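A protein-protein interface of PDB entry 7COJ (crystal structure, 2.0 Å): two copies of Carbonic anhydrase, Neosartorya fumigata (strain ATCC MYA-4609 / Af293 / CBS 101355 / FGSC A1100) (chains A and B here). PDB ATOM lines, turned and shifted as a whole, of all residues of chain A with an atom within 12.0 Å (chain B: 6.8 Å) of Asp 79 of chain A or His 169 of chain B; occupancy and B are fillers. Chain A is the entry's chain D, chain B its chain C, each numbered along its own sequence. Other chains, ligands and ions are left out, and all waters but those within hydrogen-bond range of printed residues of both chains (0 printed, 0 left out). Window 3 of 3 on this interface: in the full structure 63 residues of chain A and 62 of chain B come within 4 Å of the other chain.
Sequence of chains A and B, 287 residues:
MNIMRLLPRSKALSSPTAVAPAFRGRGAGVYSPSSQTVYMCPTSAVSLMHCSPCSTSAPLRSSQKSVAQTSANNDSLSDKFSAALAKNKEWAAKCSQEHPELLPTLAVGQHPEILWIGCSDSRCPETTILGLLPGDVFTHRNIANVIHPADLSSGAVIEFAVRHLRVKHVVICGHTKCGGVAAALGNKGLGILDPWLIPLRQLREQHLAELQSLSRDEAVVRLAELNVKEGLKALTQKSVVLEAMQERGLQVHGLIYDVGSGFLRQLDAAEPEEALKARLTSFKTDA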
ATOM      1  N   ASP A  79      17.680 -25.179   4.034  1.00  0.00           N
ATOM      2  CA  ASP A  79      16.878 -25.918   3.031  1.00  0.00           C
ATOM      3  C   ASP A  79      15.546 -26.339   3.678  1.00  0.00           C
ATOM      4  O   ASP A  79      15.551 -27.240   4.537  1.00  0.00           O
ATOM      5  CB  ASP A  79      17.698 -27.073   2.451  1.00  0.00           C
ATOM      6  CG  ASP A  79      16.920 -27.952   1.483  1.00  0.00           C
ATOM      7  OD1 ASP A  79      15.711 -27.754   1.361  1.00  0.00           O
ATOM      8  OD2 ASP A  79      17.526 -28.847   0.880  1.00  0.00           O
ATOM      9  N   LYS A  80      14.447 -25.694   3.273  1.00  0.00           N
ATOM     10  CA  LYS A  80      13.067 -25.917   3.782  1.00  0.00           C
ATOM     11  C   LYS A  80      12.621 -27.365   3.538  1.00  0.00           C
ATOM     12  O   LYS A  80      11.849 -27.906   4.349  1.00  0.00           O
ATOM     13  CB  LYS A  80      12.076 -25.004   3.051  1.00  0.00           C
ATOM     14  CG  LYS A  80      11.102 -24.259   3.943  1.00  0.00           C
ATOM     15  CD  LYS A  80      11.819 -23.310   4.843  1.00  0.00           C
ATOM     16  CE  LYS A  80      10.890 -22.243   5.371  1.00  0.00           C
ATOM     17  NZ  LYS A  80      11.679 -21.156   5.976  1.00  0.00           N
ATOM     18  N   PHE A  81      13.069 -27.954   2.430  1.00  0.00           N
ATOM     19  CA  PHE A  81      12.684 -29.325   2.026  1.00  0.00           C
ATOM     20  C   PHE A  81      13.357 -30.342   2.959  1.00  0.00           C
ATOM     21  O   PHE A  81      12.639 -31.149   3.536  1.00  0.00           O
ATOM     22  CB  PHE A  81      12.993 -29.582   0.549  1.00  0.00           C
ATOM     23  CG  PHE A  81      12.735 -31.008   0.156  1.00  0.00           C
ATOM     24  CD1 PHE A  81      11.435 -31.485   0.029  1.00  0.00           C
ATOM     25  CD2 PHE A  81      13.796 -31.874  -0.024  1.00  0.00           C
ATOM     26  CE1 PHE A  81      11.211 -32.800  -0.324  1.00  0.00           C
ATOM     27  CE2 PHE A  81      13.567 -33.185  -0.412  1.00  0.00           C
ATOM     28  CZ  PHE A  81      12.277 -33.643  -0.555  1.00  0.00           C
ATOM     29  N   SER A  82      14.678 -30.298   3.126  1.00  0.00           N
ATOM     30  CA  SER A  82      15.385 -31.218   4.059  1.00  0.00           C
ATOM     31  C   SER A  82      14.895 -30.957   5.492  1.00  0.00           C
ATOM     32  O   SER A  82      14.690 -31.936   6.218  1.00  0.00           O
ATOM     33  CB  SER A  82      16.887 -31.141   3.937  1.00  0.00           C
ATOM     34  OG  SER A  82      17.303 -29.799   4.072  1.00  0.00           O
ATOM     35  N   ALA A  83      14.578 -29.718   5.861  1.00  0.00           N
ATOM     36  CA  ALA A  83      14.038 -29.407   7.206  1.00  0.00           C
ATOM     37  C   ALA A  83      12.666 -30.078   7.370  1.00  0.00           C
ATOM     38  O   ALA A  83      12.361 -30.595   8.471  1.00  0.00           O
ATOM     39  CB  ALA A  83      13.960 -27.911   7.431  1.00  0.00           C
ATOM     40  N   ALA A  84      11.854 -30.092   6.308  1.00  0.00           N
ATOM     41  CA  ALA A  84      10.494 -30.665   6.338  1.00  0.00           C
ATOM     42  C   ALA A  84      10.605 -32.185   6.472  1.00  0.00           C
ATOM     43  O   ALA A  84       9.808 -32.741   7.222  1.00  0.00           O
ATOM     44  CB  ALA A  84       9.723 -30.261   5.108  1.00  0.00           C
ATOM     45  N   LEU A  85      11.550 -32.830   5.781  1.00  0.00           N
ATOM     46  CA  LEU A  85      11.734 -34.302   5.881  1.00  0.00           C
ATOM     47  C   LEU A  85      12.133 -34.651   7.319  1.00  0.00           C
ATOM     48  O   LEU A  85      11.627 -35.632   7.839  1.00  0.00           O
ATOM     49  CB  LEU A  85      12.780 -34.793   4.888  1.00  0.00           C
ATOM     50  CG  LEU A  85      12.396 -34.700   3.409  1.00  0.00           C
ATOM     51  CD1 LEU A  85      13.427 -35.393   2.551  1.00  0.00           C
ATOM     52  CD2 LEU A  85      11.015 -35.262   3.150  1.00  0.00           C
ATOM     53  N   ALA A  86      12.991 -33.858   7.961  1.00  0.00           N
ATOM     54  CA  ALA A  86      13.395 -34.095   9.368  1.00  0.00           C
ATOM     55  C   ALA A  86      12.168 -33.955  10.283  1.00  0.00           C
ATOM     56  O   ALA A  86      11.935 -34.832  11.133  1.00  0.00           O
ATOM     57  CB  ALA A  86      14.530 -33.169   9.750  1.00  0.00           C
ATOM     58  N   LYS A  87      11.333 -32.937  10.067  1.00  0.00           N
ATOM     59  CA  LYS A  87      10.129 -32.709  10.882  1.00  0.00           C
ATOM     60  C   LYS A  87       9.123 -33.825  10.651  1.00  0.00           C
ATOM     61  O   LYS A  87       8.463 -34.219  11.616  1.00  0.00           O
ATOM     62  CB  LYS A  87       9.538 -31.334  10.555  1.00  0.00           C
ATOM     63  CG  LYS A  87      10.270 -30.187  11.215  1.00  0.00           C
ATOM     64  CD  LYS A  87       9.726 -28.870  10.787  1.00  0.00           C
ATOM     65  CE  LYS A  87      10.270 -27.707  11.583  1.00  0.00           C
ATOM     66  NZ  LYS A  87       9.794 -26.444  10.986  1.00  0.00           N
ATOM     67  N   ASN A  88       9.045 -34.353   9.423  1.00  0.00           N
ATOM     68  CA  ASN A  88       8.181 -35.527   9.141  1.00  0.00           C
ATOM     69  C   ASN A  88       8.620 -36.682  10.054  1.00  0.00           C
ATOM     70  O   ASN A  88       7.755 -37.330  10.640  1.00  0.00           O
ATOM     71  CB  ASN A  88       8.214 -35.921   7.662  1.00  0.00           C
ATOM     72  CG  ASN A  88       7.768 -37.342   7.425  1.00  0.00           C
ATOM     73  OD1 ASN A  88       6.607 -37.689   7.618  1.00  0.00           O
ATOM     74  ND2 ASN A  88       8.696 -38.200   7.045  1.00  0.00           N
ATOM     75  N   LYS A  89       9.916 -36.994  10.089  1.00  0.00           N
ATOM     76  CA  LYS A  89      10.405 -38.181  10.833  1.00  0.00           C
ATOM     77  C   LYS A  89      10.075 -37.989  12.317  1.00  0.00           C
ATOM     78  O   LYS A  89       9.598 -38.973  12.959  1.00  0.00           O
ATOM     79  CB  LYS A  89      11.907 -38.415  10.643  1.00  0.00           C
ATOM     80  CG  LYS A  89      12.458 -38.432   9.233  1.00  0.00           C
ATOM     81  CD  LYS A  89      11.875 -39.442   8.280  1.00  0.00           C
ATOM     82  CE  LYS A  89      12.805 -39.741   7.107  1.00  0.00           C
ATOM     83  NZ  LYS A  89      13.191 -38.537   6.328  1.00  0.00           N
ATOM     84  N   SER A 120      -5.989 -24.540  -3.065  1.00  0.00           N
ATOM     85  CA  SER A 120      -4.554 -24.924  -2.944  1.00  0.00           C
ATOM     86  C   SER A 120      -3.813 -23.949  -2.017  1.00  0.00           C
ATOM     87  O   SER A 120      -2.708 -24.276  -1.561  1.00  0.00           O
ATOM     88  CB  SER A 120      -3.947 -24.941  -4.311  1.00  0.00           C
ATOM     89  OG  SER A 120      -4.514 -25.977  -5.074  1.00  0.00           O
ATOM     90  N   SER A 122      -1.814 -22.090   0.538  1.00  0.00           N
ATOM     91  CA  SER A 122      -0.998 -22.712   1.609  1.00  0.00           C
ATOM     92  C   SER A 122      -1.639 -22.449   2.983  1.00  0.00           C
ATOM     93  O   SER A 122      -1.335 -23.181   3.924  1.00  0.00           O
ATOM     94  CB  SER A 122       0.413 -22.218   1.608  1.00  0.00           C
ATOM     95  OG  SER A 122       0.440 -20.808   1.841  1.00  0.00           O
ATOM     96  N   GLU B 113       7.251 -22.011   0.574  1.00  0.00           N
ATOM     97  CA  GLU B 113       8.463 -22.351  -0.206  1.00  0.00           C
ATOM     98  C   GLU B 113       8.311 -23.707  -0.882  1.00  0.00           C
ATOM     99  O   GLU B 113       9.236 -24.083  -1.669  1.00  0.00           O
ATOM    100  CB  GLU B 113       9.681 -22.307   0.720  1.00  0.00           C
ATOM    101  CG  GLU B 113       9.899 -20.905   1.280  1.00  0.00           C
ATOM    102  CD  GLU B 113      11.295 -20.575   1.797  1.00  0.00           C
ATOM    103  OE1 GLU B 113      12.245 -21.337   1.515  1.00  0.00           O
ATOM    104  OE2 GLU B 113      11.417 -19.530   2.479  1.00  0.00           O
ATOM    105  N   ILE B 114       7.204 -24.414  -0.620  1.00  0.00           N
ATOM    106  CA  ILE B 114       6.976 -25.805  -1.105  1.00  0.00           C
ATOM    107  C   ILE B 114       5.639 -25.859  -1.837  1.00  0.00           C
ATOM    108  O   ILE B 114       4.638 -25.369  -1.271  1.00  0.00           O
ATOM    109  CB  ILE B 114       7.047 -26.824   0.047  1.00  0.00           C
ATOM    110  CG1 ILE B 114       8.441 -26.840   0.681  1.00  0.00           C
ATOM    111  CG2 ILE B 114       6.655 -28.224  -0.430  1.00  0.00           C
ATOM    112  CD1 ILE B 114       8.501 -27.511   2.034  1.00  0.00           C
ATOM    113  N   LEU B 115       5.651 -26.431  -3.048  1.00  0.00           N
ATOM    114  CA  LEU B 115       4.451 -26.946  -3.736  1.00  0.00           C
ATOM    115  C   LEU B 115       4.450 -28.454  -3.542  1.00  0.00           C
ATOM    116  O   LEU B 115       5.463 -29.130  -3.888  1.00  0.00           O
ATOM    117  CB  LEU B 115       4.456 -26.587  -5.226  1.00  0.00           C
ATOM    118  CG  LEU B 115       3.458 -27.375  -6.087  1.00  0.00           C
ATOM    119  CD1 LEU B 115       2.014 -27.145  -5.637  1.00  0.00           C
ATOM    120  CD2 LEU B 115       3.604 -27.045  -7.545  1.00  0.00           C
ATOM    121  N   TRP B 116       3.381 -28.951  -2.967  1.00  0.00           N
ATOM    122  CA  TRP B 116       3.125 -30.391  -2.763  1.00  0.00           C
ATOM    123  C   TRP B 116       2.041 -30.835  -3.745  1.00  0.00           C
ATOM    124  O   TRP B 116       0.924 -30.246  -3.733  1.00  0.00           O
ATOM    125  CB  TRP B 116       2.695 -30.602  -1.329  1.00  0.00           C
ATOM    126  CG  TRP B 116       2.322 -32.002  -0.957  1.00  0.00           C
ATOM    127  CD1 TRP B 116       1.117 -32.618  -1.144  1.00  0.00           C
ATOM    128  CD2 TRP B 116       3.128 -32.905  -0.203  1.00  0.00           C
ATOM    129  NE1 TRP B 116       1.141 -33.864  -0.591  1.00  0.00           N
ATOM    130  CE2 TRP B 116       2.360 -34.058   0.001  1.00  0.00           C
ATOM    131  CE3 TRP B 116       4.417 -32.845   0.320  1.00  0.00           C
ATOM    132  CZ2 TRP B 116       2.841 -35.145   0.714  1.00  0.00           C
ATOM    133  CZ3 TRP B 116       4.899 -33.925   1.017  1.00  0.00           C
ATOM    134  CH2 TRP B 116       4.124 -35.052   1.204  1.00  0.00           C
ATOM    135  N   ARG B 166       6.780 -18.273  -6.459  1.00  0.00           N
ATOM    136  CA  ARG B 166       8.236 -18.592  -6.553  1.00  0.00           C
ATOM    137  C   ARG B 166       8.610 -19.617  -5.484  1.00  0.00           C
ATOM    138  O   ARG B 166       9.593 -19.447  -4.769  1.00  0.00           O
ATOM    139  CB  ARG B 166       9.049 -17.296  -6.512  1.00  0.00           C
ATOM    140  CG  ARG B 166       8.802 -16.429  -7.744  1.00  0.00           C
ATOM    141  CD  ARG B 166       9.373 -15.021  -7.644  1.00  0.00           C
ATOM    142  NE  ARG B 166      10.823 -15.054  -7.494  1.00  0.00           N
ATOM    143  CZ  ARG B 166      11.705 -15.140  -8.492  1.00  0.00           C
ATOM    144  NH1 ARG B 166      11.299 -15.229  -9.745  1.00  0.00           N
ATOM    145  NH2 ARG B 166      13.008 -15.159  -8.232  1.00  0.00           N
ATOM    146  N   VAL B 167       7.871 -20.726  -5.407  1.00  0.00           N
ATOM    147  CA  VAL B 167       8.262 -21.803  -4.470  1.00  0.00           C
ATOM    148  C   VAL B 167       9.684 -22.257  -4.853  1.00  0.00           C
ATOM    149  O   VAL B 167      10.027 -22.243  -6.030  1.00  0.00           O
ATOM    150  CB  VAL B 167       7.264 -22.981  -4.483  1.00  0.00           C
ATOM    151  CG1 VAL B 167       5.901 -22.542  -3.976  1.00  0.00           C
ATOM    152  CG2 VAL B 167       7.158 -23.619  -5.855  1.00  0.00           C
ATOM    153  N   LYS B 168      10.442 -22.699  -3.879  1.00  0.00           N
ATOM    154  CA  LYS B 168      11.846 -23.174  -4.078  1.00  0.00           C
ATOM    155  C   LYS B 168      11.834 -24.676  -4.322  1.00  0.00           C
ATOM    156  O   LYS B 168      12.808 -25.188  -4.878  1.00  0.00           O
ATOM    157  CB  LYS B 168      12.686 -22.833  -2.842  1.00  0.00           C
ATOM    158  CG  LYS B 168      12.839 -21.333  -2.587  1.00  0.00           C
ATOM    159  CD  LYS B 168      13.822 -21.016  -1.475  1.00  0.00           C
ATOM    160  CE  LYS B 168      14.177 -19.548  -1.351  1.00  0.00           C
ATOM    161  NZ  LYS B 168      12.993 -18.707  -1.045  1.00  0.00           N
ATOM    162  N   HIS B 169      10.753 -25.367  -3.949  1.00  0.00           N
ATOM    163  CA  HIS B 169      10.672 -26.846  -4.032  1.00  0.00           C
ATOM    164  C   HIS B 169       9.323 -27.285  -4.571  1.00  0.00           C
ATOM    165  O   HIS B 169       8.299 -26.772  -4.068  1.00  0.00           O
ATOM    166  CB  HIS B 169      10.867 -27.467  -2.646  1.00  0.00           C
ATOM    167  CG  HIS B 169      12.174 -27.117  -2.034  1.00  0.00           C
ATOM    168  ND1 HIS B 169      13.351 -27.742  -2.406  1.00  0.00           N
ATOM    169  CD2 HIS B 169      12.503 -26.172  -1.124  1.00  0.00           C
ATOM    170  CE1 HIS B 169      14.348 -27.221  -1.720  1.00  0.00           C
ATOM    171  NE2 HIS B 169      13.864 -26.256  -0.941  1.00  0.00           N
ATOM    172  N   VAL B 170       9.330 -28.166  -5.567  1.00  0.00           N
ATOM    173  CA  VAL B 170       8.115 -28.887  -6.002  1.00  0.00           C
ATOM    174  C   VAL B 170       8.282 -30.348  -5.622  1.00  0.00           C
ATOM    175  O   VAL B 170       9.299 -30.975  -6.023  1.00  0.00           O
ATOM    176  CB  VAL B 170       7.833 -28.739  -7.503  1.00  0.00           C
ATOM    177  CG1 VAL B 170       6.581 -29.530  -7.854  1.00  0.00           C
ATOM    178  CG2 VAL B 170       7.710 -27.293  -7.927  1.00  0.00           C
ATOM    179  N   VAL B 171       7.352 -30.860  -4.843  1.00  0.00           N
ATOM    180  CA  VAL B 171       7.387 -32.252  -4.328  1.00  0.00           C
ATOM    181  C   VAL B 171       6.243 -33.015  -4.987  1.00  0.00           C
ATOM    182  O   VAL B 171       5.074 -32.552  -4.869  1.00  0.00           O
ATOM    183  CB  VAL B 171       7.262 -32.260  -2.791  1.00  0.00           C
ATOM    184  CG1 VAL B 171       7.200 -33.666  -2.251  1.00  0.00           C
ATOM    185  CG2 VAL B 171       8.403 -31.501  -2.128  1.00  0.00           C
ATOM    186  N   ARG B 248      16.686 -19.768 -11.084  1.00  0.00           N
ATOM    187  CA  ARG B 248      16.695 -19.553  -9.610  1.00  0.00           C
ATOM    188  C   ARG B 248      16.865 -20.860  -8.833  1.00  0.00           C
ATOM    189  O   ARG B 248      16.681 -20.821  -7.640  1.00  0.00           O
ATOM    190  CB  ARG B 248      15.456 -18.744  -9.199  1.00  0.00           C
ATOM    191  CG  ARG B 248      14.112 -19.413  -9.437  1.00  0.00           C
ATOM    192  CD  ARG B 248      12.946 -18.518  -9.003  1.00  0.00           C
ATOM    193  NE  ARG B 248      11.640 -19.162  -9.145  1.00  0.00           N
ATOM    194  CZ  ARG B 248      11.172 -20.121  -8.326  1.00  0.00           C
ATOM    195  NH1 ARG B 248      11.880 -20.500  -7.273  1.00  0.00           N
ATOM    196  NH2 ARG B 248       9.994 -20.692  -8.546  1.00  0.00           N
ATOM    197  N   GLY B 249      17.279 -21.943  -9.479  1.00  0.00           N
ATOM    198  CA  GLY B 249      17.619 -23.208  -8.809  1.00  0.00           C
ATOM    199  C   GLY B 249      16.405 -23.851  -8.147  1.00  0.00           C
ATOM    200  O   GLY B 249      16.593 -24.525  -7.142  1.00  0.00           O
ATOM    201  N   LEU B 250      15.208 -23.678  -8.697  1.00  0.00           N
ATOM    202  CA  LEU B 250      14.027 -24.454  -8.227  1.00  0.00           C
ATOM    203  C   LEU B 250      14.449 -25.923  -8.226  1.00  0.00           C
ATOM    204  O   LEU B 250      15.081 -26.363  -9.199  1.00  0.00           O
ATOM    205  CB  LEU B 250      12.844 -24.241  -9.170  1.00  0.00           C
ATOM    206  CG  LEU B 250      11.655 -25.185  -8.939  1.00  0.00           C
ATOM    207  CD1 LEU B 250      10.890 -24.737  -7.734  1.00  0.00           C
ATOM    208  CD2 LEU B 250      10.727 -25.239 -10.117  1.00  0.00           C
ATOM    209  N   GLN B 251      14.083 -26.664  -7.188  1.00  0.00           N
ATOM    210  CA  GLN B 251      14.352 -28.115  -7.097  1.00  0.00           C
ATOM    211  C   GLN B 251      13.027 -28.884  -7.160  1.00  0.00           C
ATOM    212  O   GLN B 251      11.983 -28.389  -6.654  1.00  0.00           O
ATOM    213  CB  GLN B 251      15.102 -28.441  -5.803  1.00  0.00           C
ATOM    214  CG  GLN B 251      16.504 -27.862  -5.752  1.00  0.00           C
ATOM    215  CD  GLN B 251      17.190 -28.127  -4.442  1.00  0.00           C
ATOM    216  OE1 GLN B 251      16.779 -28.956  -3.642  1.00  0.00           O
ATOM    217  NE2 GLN B 251      18.323 -27.481  -4.280  1.00  0.00           N
ATOM    218  N   VAL B 252      13.081 -30.079  -7.734  1.00  0.00           N
ATOM    219  CA  VAL B 252      11.916 -30.995  -7.801  1.00  0.00           C
ATOM    220  C   VAL B 252      12.293 -32.284  -7.081  1.00  0.00           C
ATOM    221  O   VAL B 252      13.475 -32.687  -7.149  1.00  0.00           O
ATOM    222  CB  VAL B 252      11.501 -31.208  -9.261  1.00  0.00           C
ATOM    223  CG1 VAL B 252      11.186 -29.869  -9.918  1.00  0.00           C
ATOM    224  CG2 VAL B 252      12.534 -31.983 -10.075  1.00  0.00           C
ATOM    225  N   HIS B 253      11.337 -32.910  -6.408  1.00  0.00           N
ATOM    226  CA  HIS B 253      11.594 -34.061  -5.526  1.00  0.00           C
ATOM    227  C   HIS B 253      10.467 -35.069  -5.673  1.00  0.00           C
ATOM    228  O   HIS B 253       9.291 -34.642  -5.725  1.00  0.00           O
ATOM    229  CB  HIS B 253      11.706 -33.623  -4.056  1.00  0.00           C
ATOM    230  CG  HIS B 253      12.535 -32.412  -3.825  1.00  0.00           C
ATOM    231  ND1 HIS B 253      13.863 -32.489  -3.545  1.00  0.00           N
ATOM    232  CD2 HIS B 253      12.210 -31.101  -3.749  1.00  0.00           C
ATOM    233  CE1 HIS B 253      14.353 -31.274  -3.373  1.00  0.00           C
ATOM    234  NE2 HIS B 253      13.356 -30.411  -3.466  1.00  0.00           N
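NZ of Lys 80 of chain A is in salt-bridge range of OE2 of Glu 113 of chain B (3.9 Å). A ring nitrogen (NE2) of His 169 of chain B sits at hydrogen-bond distance from the side-chain carboxylate (OD1) of Asp 79 of chain A, 3.3 Å away.
The side-chain carboxylate (OD1) of Asp 79 of chain A is in hydrogen-bond range of the backbone NH (N) of Phe 81 of chain A (2.9 Å). The side-chain carboxylate of Glu 113 of chain B lies within salt-bridge range of the side-chain amino group of Lys 168 of chain B (3.7 Å). O of Glu 113 of chain B sits at hydrogen-bond distance from N of His 169 of chain B (3.0 Å). O of Leu 115 of chain B is in hydrogen-bond range of N of Val 171 of chain B, 2.7 Å away. N of His 253 of chain B lies within hydrogen-bond range of O of Val 170 of chain B (2.8 Å). The backbone NH (N) of Leu 115 of chain B sits at hydrogen-bond distance from the backbone carbonyl oxygen (O) of His 169 of chain B (2.9 Å).
Among the printed residues, merely in contact across the chains: Phe 81 of chain A with His 253 of chain B (3.2 Å), Phe 81 of chain A with His 169 of chain B (3.5 Å) and Phe 81 of chain A with Val 171 of chain B (3.6 Å).
Of chain A, only Asp 79 (3.3 Å) and Phe 81 (3.5 Å) come within 4 Å of His 169 of chain B. No residue of chain A comes within 4 Å of Ile 114 of chain B. No residue of chain A comes within 4 Å of Leu 115 of chain B. No residue of chain A comes within 4 Å of Lys 168 of chain B. No residue of chain A comes within 4 Å of Val 170 of chain B. Val 171 of chain B touches just one residue of chain A: Phe 81 (3.6 Å). Leu 250 of chain B touches none of the printed residues of chain A. Gln 251 of chain B touches none of the printed residues of chain A. No residue of chain A comes within 4 Å of Val 252 of chain B. Of the printed residues of chain B, Phe 81 of chain A touches His 169, Val 171 and His 253. Of the printed residues of chain B, Lys 80 of chain A touches Glu 113. Ser 120 of chain A touches none of the printed residues of chain B. Arg 166 of chain B touches none of the printed residues of chain A.
Printed residues of chain B that touch a printed residue of chain A: Glu 113, His 169, Val 171 and His 253. Hydrophobic or aromatic side chains of chain B that line the printed part of chain A: His 169, Val 171 and His 253. Along chain B the printed residues that touch a printed residue of chain A span positions 113 to 253. Among the printed residues, 5 pairs touch across the chains.
No position is printed for both chains. Of the 5 pairs that touch across the chains among the printed residues, none has its exchanged pair printed and touching as well.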
